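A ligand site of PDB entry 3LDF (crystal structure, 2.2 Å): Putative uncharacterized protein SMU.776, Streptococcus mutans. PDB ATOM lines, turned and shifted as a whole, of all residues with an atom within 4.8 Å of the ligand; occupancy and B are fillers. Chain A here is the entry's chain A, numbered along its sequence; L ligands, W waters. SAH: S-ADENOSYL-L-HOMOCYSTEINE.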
ATOM      1  N   MET A 192     -35.488  19.357  25.302  1.00  0.00           N
ATOM      2  CA  MET A 192     -34.236  20.086  25.531  1.00  0.00           C
ATOM      3  C   MET A 192     -34.527  21.583  25.705  1.00  0.00           C
ATOM      4  O   MET A 192     -35.610  22.044  25.314  1.00  0.00           O
ATOM      5  CB  MET A 192     -33.315  19.950  24.300  1.00  0.00           C
ATOM      6  CG  MET A 192     -32.664  18.531  24.125  1.00  0.00           C
ATOM      7  SD  MET A 192     -31.405  18.405  22.814  1.00  0.00           S
ATOM      8  CE  MET A 192     -32.506  18.531  21.364  1.00  0.00           C
ATOM      9  N   PHE A 196     -27.241  21.917  27.868  1.00  0.00           N
ATOM     10  CA  PHE A 196     -27.004  20.879  28.840  1.00  0.00           C
ATOM     11  C   PHE A 196     -26.105  21.444  29.904  1.00  0.00           C
ATOM     12  O   PHE A 196     -24.868  21.634  29.700  1.00  0.00           O
ATOM     13  CB  PHE A 196     -26.313  19.639  28.150  1.00  0.00           C
ATOM     14  CG  PHE A 196     -27.260  18.920  27.201  1.00  0.00           C
ATOM     15  CD1 PHE A 196     -28.069  17.866  27.678  1.00  0.00           C
ATOM     16  CD2 PHE A 196     -27.431  19.387  25.881  1.00  0.00           C
ATOM     17  CE1 PHE A 196     -28.998  17.233  26.810  1.00  0.00           C
ATOM     18  CE2 PHE A 196     -28.318  18.785  25.029  1.00  0.00           C
ATOM     19  CZ  PHE A 196     -29.134  17.690  25.486  1.00  0.00           C
ATOM     20  N   GLN A 199     -22.431  20.176  31.453  1.00  0.00           N
ATOM     21  CA  GLN A 199     -21.144  20.461  30.827  1.00  0.00           C
ATOM     22  C   GLN A 199     -20.584  21.819  31.262  1.00  0.00           C
ATOM     23  O   GLN A 199     -19.578  22.320  30.708  1.00  0.00           O
ATOM     24  CB  GLN A 199     -21.265  20.348  29.274  1.00  0.00           C
ATOM     25  CG  GLN A 199     -21.316  18.816  28.909  1.00  0.00           C
ATOM     26  CD  GLN A 199     -21.974  18.596  27.586  1.00  0.00           C
ATOM     27  OE1 GLN A 199     -22.844  19.354  27.208  1.00  0.00           O
ATOM     28  NE2 GLN A 199     -21.485  17.616  26.816  1.00  0.00           N
ATOM     29  N   LEU A 219     -18.548  19.819  16.859  1.00  0.00           N
ATOM     30  CA  LEU A 219     -19.388  18.851  16.097  1.00  0.00           C
ATOM     31  C   LEU A 219     -20.626  18.426  16.916  1.00  0.00           C
ATOM     32  O   LEU A 219     -20.495  18.192  18.140  1.00  0.00           O
ATOM     33  CB  LEU A 219     -18.558  17.609  15.761  1.00  0.00           C
ATOM     34  CG  LEU A 219     -17.315  17.858  14.869  1.00  0.00           C
ATOM     35  CD1 LEU A 219     -16.507  16.581  14.586  1.00  0.00           C
ATOM     36  CD2 LEU A 219     -17.784  18.420  13.484  1.00  0.00           C
ATOM     37  N   PHE A 220     -21.769  18.281  16.252  1.00  0.00           N
ATOM     38  CA  PHE A 220     -23.117  18.105  16.875  1.00  0.00           C
ATOM     39  C   PHE A 220     -23.363  19.253  17.817  1.00  0.00           C
ATOM     40  O   PHE A 220     -23.674  19.011  18.981  1.00  0.00           O
ATOM     41  CB  PHE A 220     -23.258  16.756  17.621  1.00  0.00           C
ATOM     42  CG  PHE A 220     -22.764  15.542  16.810  1.00  0.00           C
ATOM     43  CD1 PHE A 220     -23.710  14.738  16.088  1.00  0.00           C
ATOM     44  CD2 PHE A 220     -21.417  15.195  16.763  1.00  0.00           C
ATOM     45  CE1 PHE A 220     -23.295  13.582  15.378  1.00  0.00           C
ATOM     46  CE2 PHE A 220     -20.981  14.036  16.044  1.00  0.00           C
ATOM     47  CZ  PHE A 220     -21.929  13.251  15.334  1.00  0.00           C
ATOM     48  N   SER A 221     -23.207  20.510  17.301  1.00  0.00           N
ATOM     49  CA  SER A 221     -23.088  21.686  18.162  1.00  0.00           C
ATOM     50  C   SER A 221     -24.371  22.050  18.934  1.00  0.00           C
ATOM     51  O   SER A 221     -24.275  22.642  20.030  1.00  0.00           O
ATOM     52  CB  SER A 221     -22.571  22.873  17.369  1.00  0.00           C
ATOM     53  OG  SER A 221     -23.360  23.062  16.222  1.00  0.00           O
ATOM     54  N   TYR A 222     -25.558  21.669  18.381  1.00  0.00           N
ATOM     55  CA  TYR A 222     -26.869  22.002  18.957  1.00  0.00           C
ATOM     56  C   TYR A 222     -27.126  23.532  18.888  1.00  0.00           C
ATOM     57  O   TYR A 222     -27.594  24.055  17.851  1.00  0.00           O
ATOM     58  CB  TYR A 222     -27.036  21.394  20.387  1.00  0.00           C
ATOM     59  CG  TYR A 222     -28.386  21.668  21.011  1.00  0.00           C
ATOM     60  CD1 TYR A 222     -29.562  21.646  20.233  1.00  0.00           C
ATOM     61  CD2 TYR A 222     -28.493  21.996  22.384  1.00  0.00           C
ATOM     62  CE1 TYR A 222     -30.837  21.940  20.782  1.00  0.00           C
ATOM     63  CE2 TYR A 222     -29.790  22.259  22.963  1.00  0.00           C
ATOM     64  CZ  TYR A 222     -30.925  22.255  22.136  1.00  0.00           C
ATOM     65  OH  TYR A 222     -32.138  22.548  22.668  1.00  0.00           O
ATOM     66  N   THR A 223     -26.756  24.277  19.946  1.00  0.00           N
ATOM     67  CA  THR A 223     -26.912  25.747  19.909  1.00  0.00           C
ATOM     68  C   THR A 223     -25.528  26.399  20.122  1.00  0.00           C
ATOM     69  O   THR A 223     -25.423  27.574  20.520  1.00  0.00           O
ATOM     70  CB  THR A 223     -27.908  26.251  20.985  1.00  0.00           C
ATOM     71  OG1 THR A 223     -27.333  26.034  22.278  1.00  0.00           O
ATOM     72  CG2 THR A 223     -29.239  25.459  20.974  1.00  0.00           C
ATOM     73  N   PHE A 226     -20.669  25.366  23.388  1.00  0.00           N
ATOM     74  CA  PHE A 226     -19.208  25.232  23.537  1.00  0.00           C
ATOM     75  C   PHE A 226     -18.410  26.318  22.739  1.00  0.00           C
ATOM     76  O   PHE A 226     -17.346  26.752  23.205  1.00  0.00           O
ATOM     77  CB  PHE A 226     -18.702  23.820  23.108  1.00  0.00           C
ATOM     78  CG  PHE A 226     -18.956  22.664  24.115  1.00  0.00           C
ATOM     79  CD1 PHE A 226     -18.474  22.712  25.423  1.00  0.00           C
ATOM     80  CD2 PHE A 226     -19.557  21.462  23.680  1.00  0.00           C
ATOM     81  CE1 PHE A 226     -18.661  21.600  26.326  1.00  0.00           C
ATOM     82  CE2 PHE A 226     -19.726  20.353  24.521  1.00  0.00           C
ATOM     83  CZ  PHE A 226     -19.314  20.410  25.859  1.00  0.00           C
ATOM     84  N   VAL A 241     -21.002  22.835  13.778  1.00  0.00           N
ATOM     85  CA  VAL A 241     -21.708  22.011  12.777  1.00  0.00           C
ATOM     86  C   VAL A 241     -22.857  21.190  13.385  1.00  0.00           C
ATOM     87  O   VAL A 241     -22.630  20.340  14.268  1.00  0.00           O
ATOM     88  CB  VAL A 241     -20.736  20.977  12.134  1.00  0.00           C
ATOM     89  CG1 VAL A 241     -21.424  20.230  10.996  1.00  0.00           C
ATOM     90  CG2 VAL A 241     -19.500  21.702  11.628  1.00  0.00           C
ATOM     91  N   ASP A 242     -24.081  21.407  12.896  1.00  0.00           N
ATOM     92  CA  ASP A 242     -25.241  20.641  13.389  1.00  0.00           C
ATOM     93  C   ASP A 242     -26.182  20.348  12.252  1.00  0.00           C
ATOM     94  O   ASP A 242     -26.314  21.120  11.293  1.00  0.00           O
ATOM     95  CB  ASP A 242     -25.974  21.422  14.500  1.00  0.00           C
ATOM     96  CG  ASP A 242     -26.955  20.584  15.252  1.00  0.00           C
ATOM     97  OD1 ASP A 242     -26.598  20.017  16.315  1.00  0.00           O
ATOM     98  OD2 ASP A 242     -28.102  20.457  14.754  1.00  0.00           O
ATOM     99  N   LEU A 243     -26.843  19.202  12.335  1.00  0.00           N
ATOM    100  CA  LEU A 243     -27.703  18.779  11.236  1.00  0.00           C
ATOM    101  C   LEU A 243     -28.943  19.675  11.163  1.00  0.00           C
ATOM    102  O   LEU A 243     -29.508  19.828  10.115  1.00  0.00           O
ATOM    103  CB  LEU A 243     -28.097  17.324  11.436  1.00  0.00           C
ATOM    104  CG  LEU A 243     -28.880  16.652  10.319  1.00  0.00           C
ATOM    105  CD1 LEU A 243     -28.054  16.533   9.010  1.00  0.00           C
ATOM    106  CD2 LEU A 243     -29.377  15.282  10.827  1.00  0.00           C
ATOM    107  N   ALA A 244     -29.368  20.266  12.289  1.00  0.00           N
ATOM    108  CA  ALA A 244     -30.696  20.883  12.378  1.00  0.00           C
ATOM    109  C   ALA A 244     -30.712  22.426  12.031  1.00  0.00           C
ATOM    110  O   ALA A 244     -29.881  23.211  12.520  1.00  0.00           O
ATOM    111  CB  ALA A 244     -31.309  20.587  13.780  1.00  0.00           C
ATOM    112  N   ARG A 246     -32.556  24.896  12.957  1.00  0.00           N
ATOM    113  CA  ARG A 246     -32.820  25.700  14.148  1.00  0.00           C
ATOM    114  C   ARG A 246     -31.486  26.158  14.814  1.00  0.00           C
ATOM    115  O   ARG A 246     -31.484  27.136  15.590  1.00  0.00           O
ATOM    116  CB  ARG A 246     -33.683  24.891  15.145  1.00  0.00           C
ATOM    117  CG  ARG A 246     -32.790  23.795  15.875  1.00  0.00           C
ATOM    118  CD  ARG A 246     -33.429  22.793  16.901  1.00  0.00           C
ATOM    119  NE  ARG A 246     -32.436  21.750  17.240  1.00  0.00           N
ATOM    120  CZ  ARG A 246     -32.707  20.484  17.664  1.00  0.00           C
ATOM    121  NH1 ARG A 246     -33.951  20.069  17.887  1.00  0.00           N
ATOM    122  NH2 ARG A 246     -31.707  19.631  17.928  1.00  0.00           N
ATOM    123  N   MET A 270     -25.404  20.984   8.509  1.00  0.00           N
ATOM    124  CA  MET A 270     -24.774  19.847   7.783  1.00  0.00           C
ATOM    125  C   MET A 270     -24.651  18.606   8.647  1.00  0.00           C
ATOM    126  O   MET A 270     -24.370  18.687   9.856  1.00  0.00           O
ATOM    127  CB  MET A 270     -23.361  20.187   7.310  1.00  0.00           C
ATOM    128  CG  MET A 270     -22.907  19.309   6.133  1.00  0.00           C
ATOM    129  SD  MET A 270     -21.315  19.704   5.322  1.00  0.00           S
ATOM    130  CE  MET A 270     -21.644  21.368   4.842  1.00  0.00           C
ATOM    131  N   ASP A 271     -24.835  17.432   8.010  1.00  0.00           N
ATOM    132  CA  ASP A 271     -24.474  16.130   8.584  1.00  0.00           C
ATOM    133  C   ASP A 271     -22.935  16.052   8.853  1.00  0.00           C
ATOM    134  O   ASP A 271     -22.101  16.354   7.977  1.00  0.00           O
ATOM    135  CB  ASP A 271     -24.944  14.982   7.669  1.00  0.00           C
ATOM    136  CG  ASP A 271     -24.708  13.575   8.294  1.00  0.00           C
ATOM    137  OD1 ASP A 271     -23.642  13.339   8.906  1.00  0.00           O
ATOM    138  OD2 ASP A 271     -25.598  12.682   8.144  1.00  0.00           O
ATOM    139  N   VAL A 272     -22.600  15.645  10.071  1.00  0.00           N
ATOM    140  CA  VAL A 272     -21.226  15.616  10.555  1.00  0.00           C
ATOM    141  C   VAL A 272     -20.368  14.731   9.682  1.00  0.00           C
ATOM    142  O   VAL A 272     -19.281  15.162   9.342  1.00  0.00           O
ATOM    143  CB  VAL A 272     -21.134  15.294  12.098  1.00  0.00           C
ATOM    144  CG1 VAL A 272     -19.802  14.607  12.496  1.00  0.00           C
ATOM    145  CG2 VAL A 272     -21.344  16.553  12.918  1.00  0.00           C
ATOM    146  N   PHE A 273     -20.857  13.536   9.275  1.00  0.00           N
ATOM    147  CA  PHE A 273     -20.156  12.692   8.252  1.00  0.00           C
ATOM    148  C   PHE A 273     -19.926  13.382   6.873  1.00  0.00           C
ATOM    149  O   PHE A 273     -18.856  13.218   6.264  1.00  0.00           O
ATOM    150  CB  PHE A 273     -20.850  11.291   8.082  1.00  0.00           C
ATOM    151  CG  PHE A 273     -20.902  10.514   9.382  1.00  0.00           C
ATOM    152  CD1 PHE A 273     -19.768   9.789   9.821  1.00  0.00           C
ATOM    153  CD2 PHE A 273     -22.030  10.567  10.220  1.00  0.00           C
ATOM    154  CE1 PHE A 273     -19.789   9.100  11.077  1.00  0.00           C
ATOM    155  CE2 PHE A 273     -22.043   9.875  11.440  1.00  0.00           C
ATOM    156  CZ  PHE A 273     -20.914   9.140  11.859  1.00  0.00           C
ATOM    157  N   ASP A 292     -19.449  15.686  20.447  1.00  0.00           N
ATOM    158  CA  ASP A 292     -20.464  15.435  21.501  1.00  0.00           C
ATOM    159  C   ASP A 292     -21.771  15.042  20.869  1.00  0.00           C
ATOM    160  O   ASP A 292     -22.699  15.804  20.865  1.00  0.00           O
ATOM    161  CB  ASP A 292     -20.608  16.669  22.402  1.00  0.00           C
ATOM    162  CG  ASP A 292     -21.470  16.404  23.618  1.00  0.00           C
ATOM    163  OD1 ASP A 292     -21.422  15.289  24.190  1.00  0.00           O
ATOM    164  OD2 ASP A 292     -22.223  17.337  24.000  1.00  0.00           O
ATOM    165  N   PRO A 294     -25.479  12.938  20.143  1.00  0.00           N
ATOM    166  CA  PRO A 294     -26.497  12.310  20.972  1.00  0.00           C
ATOM    167  C   PRO A 294     -26.210  10.784  21.060  1.00  0.00           C
ATOM    168  O   PRO A 294     -25.401  10.245  20.238  1.00  0.00           O
ATOM    169  CB  PRO A 294     -27.782  12.526  20.149  1.00  0.00           C
ATOM    170  CG  PRO A 294     -27.292  12.469  18.715  1.00  0.00           C
ATOM    171  CD  PRO A 294     -25.885  13.040  18.731  1.00  0.00           C
ATOM    172  N   ALA A 297     -29.216   8.507  17.268  1.00  0.00           N
ATOM    173  CA  ALA A 297     -29.877   9.433  16.335  1.00  0.00           C
ATOM    174  C   ALA A 297     -30.292   8.797  15.016  1.00  0.00           C
ATOM    175  O   ALA A 297     -29.655   7.860  14.521  1.00  0.00           O
ATOM    176  CB  ALA A 297     -29.047  10.689  16.095  1.00  0.00           C
HETATM  177  N   SAH L   1     -23.052  18.980  22.057  1.00  0.00           N
HETATM  178  CA  SAH L   1     -24.371  19.683  22.155  1.00  0.00           C
HETATM  179  CB  SAH L   1     -25.504  18.693  22.588  1.00  0.00           C
HETATM  180  CG  SAH L   1     -25.875  17.654  21.458  1.00  0.00           C
HETATM  181  SD  SAH L   1     -27.650  17.425  21.272  1.00  0.00           S
HETATM  182  C   SAH L   1     -24.139  20.864  23.044  1.00  0.00           C
HETATM  183  O   SAH L   1     -22.961  21.147  23.391  1.00  0.00           O
HETATM  184  OXT SAH L   1     -25.134  21.528  23.447  1.00  0.00           O
HETATM  185  C5' SAH L   1     -27.650  16.424  19.787  1.00  0.00           C
HETATM  186  C4' SAH L   1     -27.534  17.212  18.459  1.00  0.00           C
HETATM  187  O4' SAH L   1     -26.926  16.406  17.434  1.00  0.00           O
HETATM  188  C3' SAH L   1     -28.876  17.684  17.864  1.00  0.00           C
HETATM  189  O3' SAH L   1     -28.776  19.093  17.714  1.00  0.00           O
HETATM  190  C2' SAH L   1     -28.975  17.106  16.453  1.00  0.00           C
HETATM  191  O2' SAH L   1     -29.360  18.128  15.523  1.00  0.00           O
HETATM  192  C1' SAH L   1     -27.499  16.768  16.155  1.00  0.00           C
HETATM  193  N9  SAH L   1     -27.218  15.654  15.188  1.00  0.00           N
HETATM  194  C8  SAH L   1     -27.701  14.355  15.222  1.00  0.00           C
HETATM  195  N7  SAH L   1     -27.162  13.633  14.208  1.00  0.00           N
HETATM  196  C5  SAH L   1     -26.321  14.455  13.516  1.00  0.00           C
HETATM  197  C6  SAH L   1     -25.426  14.344  12.352  1.00  0.00           C
HETATM  198  N6  SAH L   1     -25.318  13.159  11.698  1.00  0.00           N
HETATM  199  N1  SAH L   1     -24.692  15.456  11.986  1.00  0.00           N
HETATM  200  C2  SAH L   1     -24.795  16.644  12.627  1.00  0.00           C
HETATM  201  N3  SAH L   1     -25.577  16.810  13.700  1.00  0.00           N
HETATM  202  C4  SAH L   1     -26.365  15.783  14.168  1.00  0.00           C
HETATM  203  O   HOH W   1     -31.651  16.952  14.393  1.00  0.00           O
HETATM  204  O   HOH W   2     -29.171  12.022  12.705  1.00  0.00           O
HETATM  205  O   HOH W   3     -21.986  23.132  21.711  1.00  0.00           O
HETATM  206  O   HOH W   4     -22.085  22.597  25.609  1.00  0.00           O
HETATM  207  O   HOH W   5     -25.012  22.546  25.851  1.00  0.00           O
HETATM  208  O   HOH W   6     -29.673  22.313  16.908  1.00  0.00           O
HETATM  209  O   HOH W   7     -25.420  24.170  22.580  1.00  0.00           O
HETATM  210  O   HOH W   8     -20.913  19.655  20.559  1.00  0.00           O
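The backbone NH (N) of Ser 221 lies within hydrogen-bond range of the backbone carbonyl oxygen (O) of Val 241 (3.1 Å). The side-chain carboxylate (OD1) of Asp 242 is in hydrogen-bond range of the backbone NH (N) of Tyr 222. NE2 of Gln 199 sits at hydrogen-bond distance from OD2 of Asp 292. The backbone carbonyl oxygen (O) of Asp 242 lies within hydrogen-bond range of the backbone NH (N) of Met 270. The backbone NH (N) of Phe 220 lies within hydrogen-bond range of the backbone carbonyl oxygen (O) of Val 241, 3.0 Å away. OD1 of Asp 271 is in hydrogen-bond range of N of Phe 273, at 2.8 Å. The side-chain carboxylate of Asp 242 lies within hydrogen-bond range of the backbone NH of Ala 244, at 2.8 Å.
Phe 196 touches the ligand. O of Ser 221 touches C of the ligand, at 3.5 Å. CD2 of Tyr 222 touches OXT of the ligand, at 3.6 Å. Phe 226 touches the ligand. CB of Ala 244 touches O2' of the ligand, at 3.6 Å. Met 270 touches the ligand. Pro 294 touches the ligand. Ala 297 touches the ligand. Within 4 Å of the ligand: Phe 196, Phe 220, Ser 221, Tyr 222, Phe 226, Asp 242, Leu 243, Ala 244, Arg 246, Met 270, Asp 271, Val 272, Asp 292, Pro 294 and Ala 297.
Water W5 lies within hydrogen-bond range of OXT of the ligand (2.6 Å) and N of Phe 196 (3.1 Å). Water W8 lies within hydrogen-bond range of a nitrogen (N) of the ligand (2.7 Å), the backbone carbonyl oxygen (O) of Leu 219 (2.9 Å) and the backbone carbonyl oxygen (O) of Phe 220 (3.2 Å). Water W3 lies within hydrogen-bond range of O of the ligand (2.8 Å), O of Ser 221 (2.9 Å) and N of Phe 226 (3.1 Å). Water W7 lies within hydrogen-bond range of OG1 of Thr 223, OXT of the ligand and O of Ser 221. Water W6 lies within hydrogen-bond range of the guanidinium group of Arg 246, the backbone carbonyl oxygen of Tyr 222, the side-chain carboxylate of Asp 242 and an oxygen (O3') of the ligand.
An oxygen (O3') of the ligand is in hydrogen-bond range of the side-chain carboxylate of Asp 242 (2.7 Å). A nitrogen (N) of the ligand lies close to the backbone carbonyl oxygen of Asp 292 (3.4 Å). N3 of the ligand lies within hydrogen-bond range of N of Leu 243, 3.0 Å away. The backbone NH (N) of Val 272 is in hydrogen-bond range of a nitrogen (N1) of the ligand. The backbone carbonyl oxygen of Phe 220 lies within hydrogen-bond range of a nitrogen (N) of the ligand. OD2 of Asp 292 is in salt-bridge range of N of the ligand (2.7 Å). NH2 of Arg 246 is in hydrogen-bond range of O3' of the ligand, at 3.0 Å. N6 of the ligand lies within hydrogen-bond range of OD1 of Asp 271.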
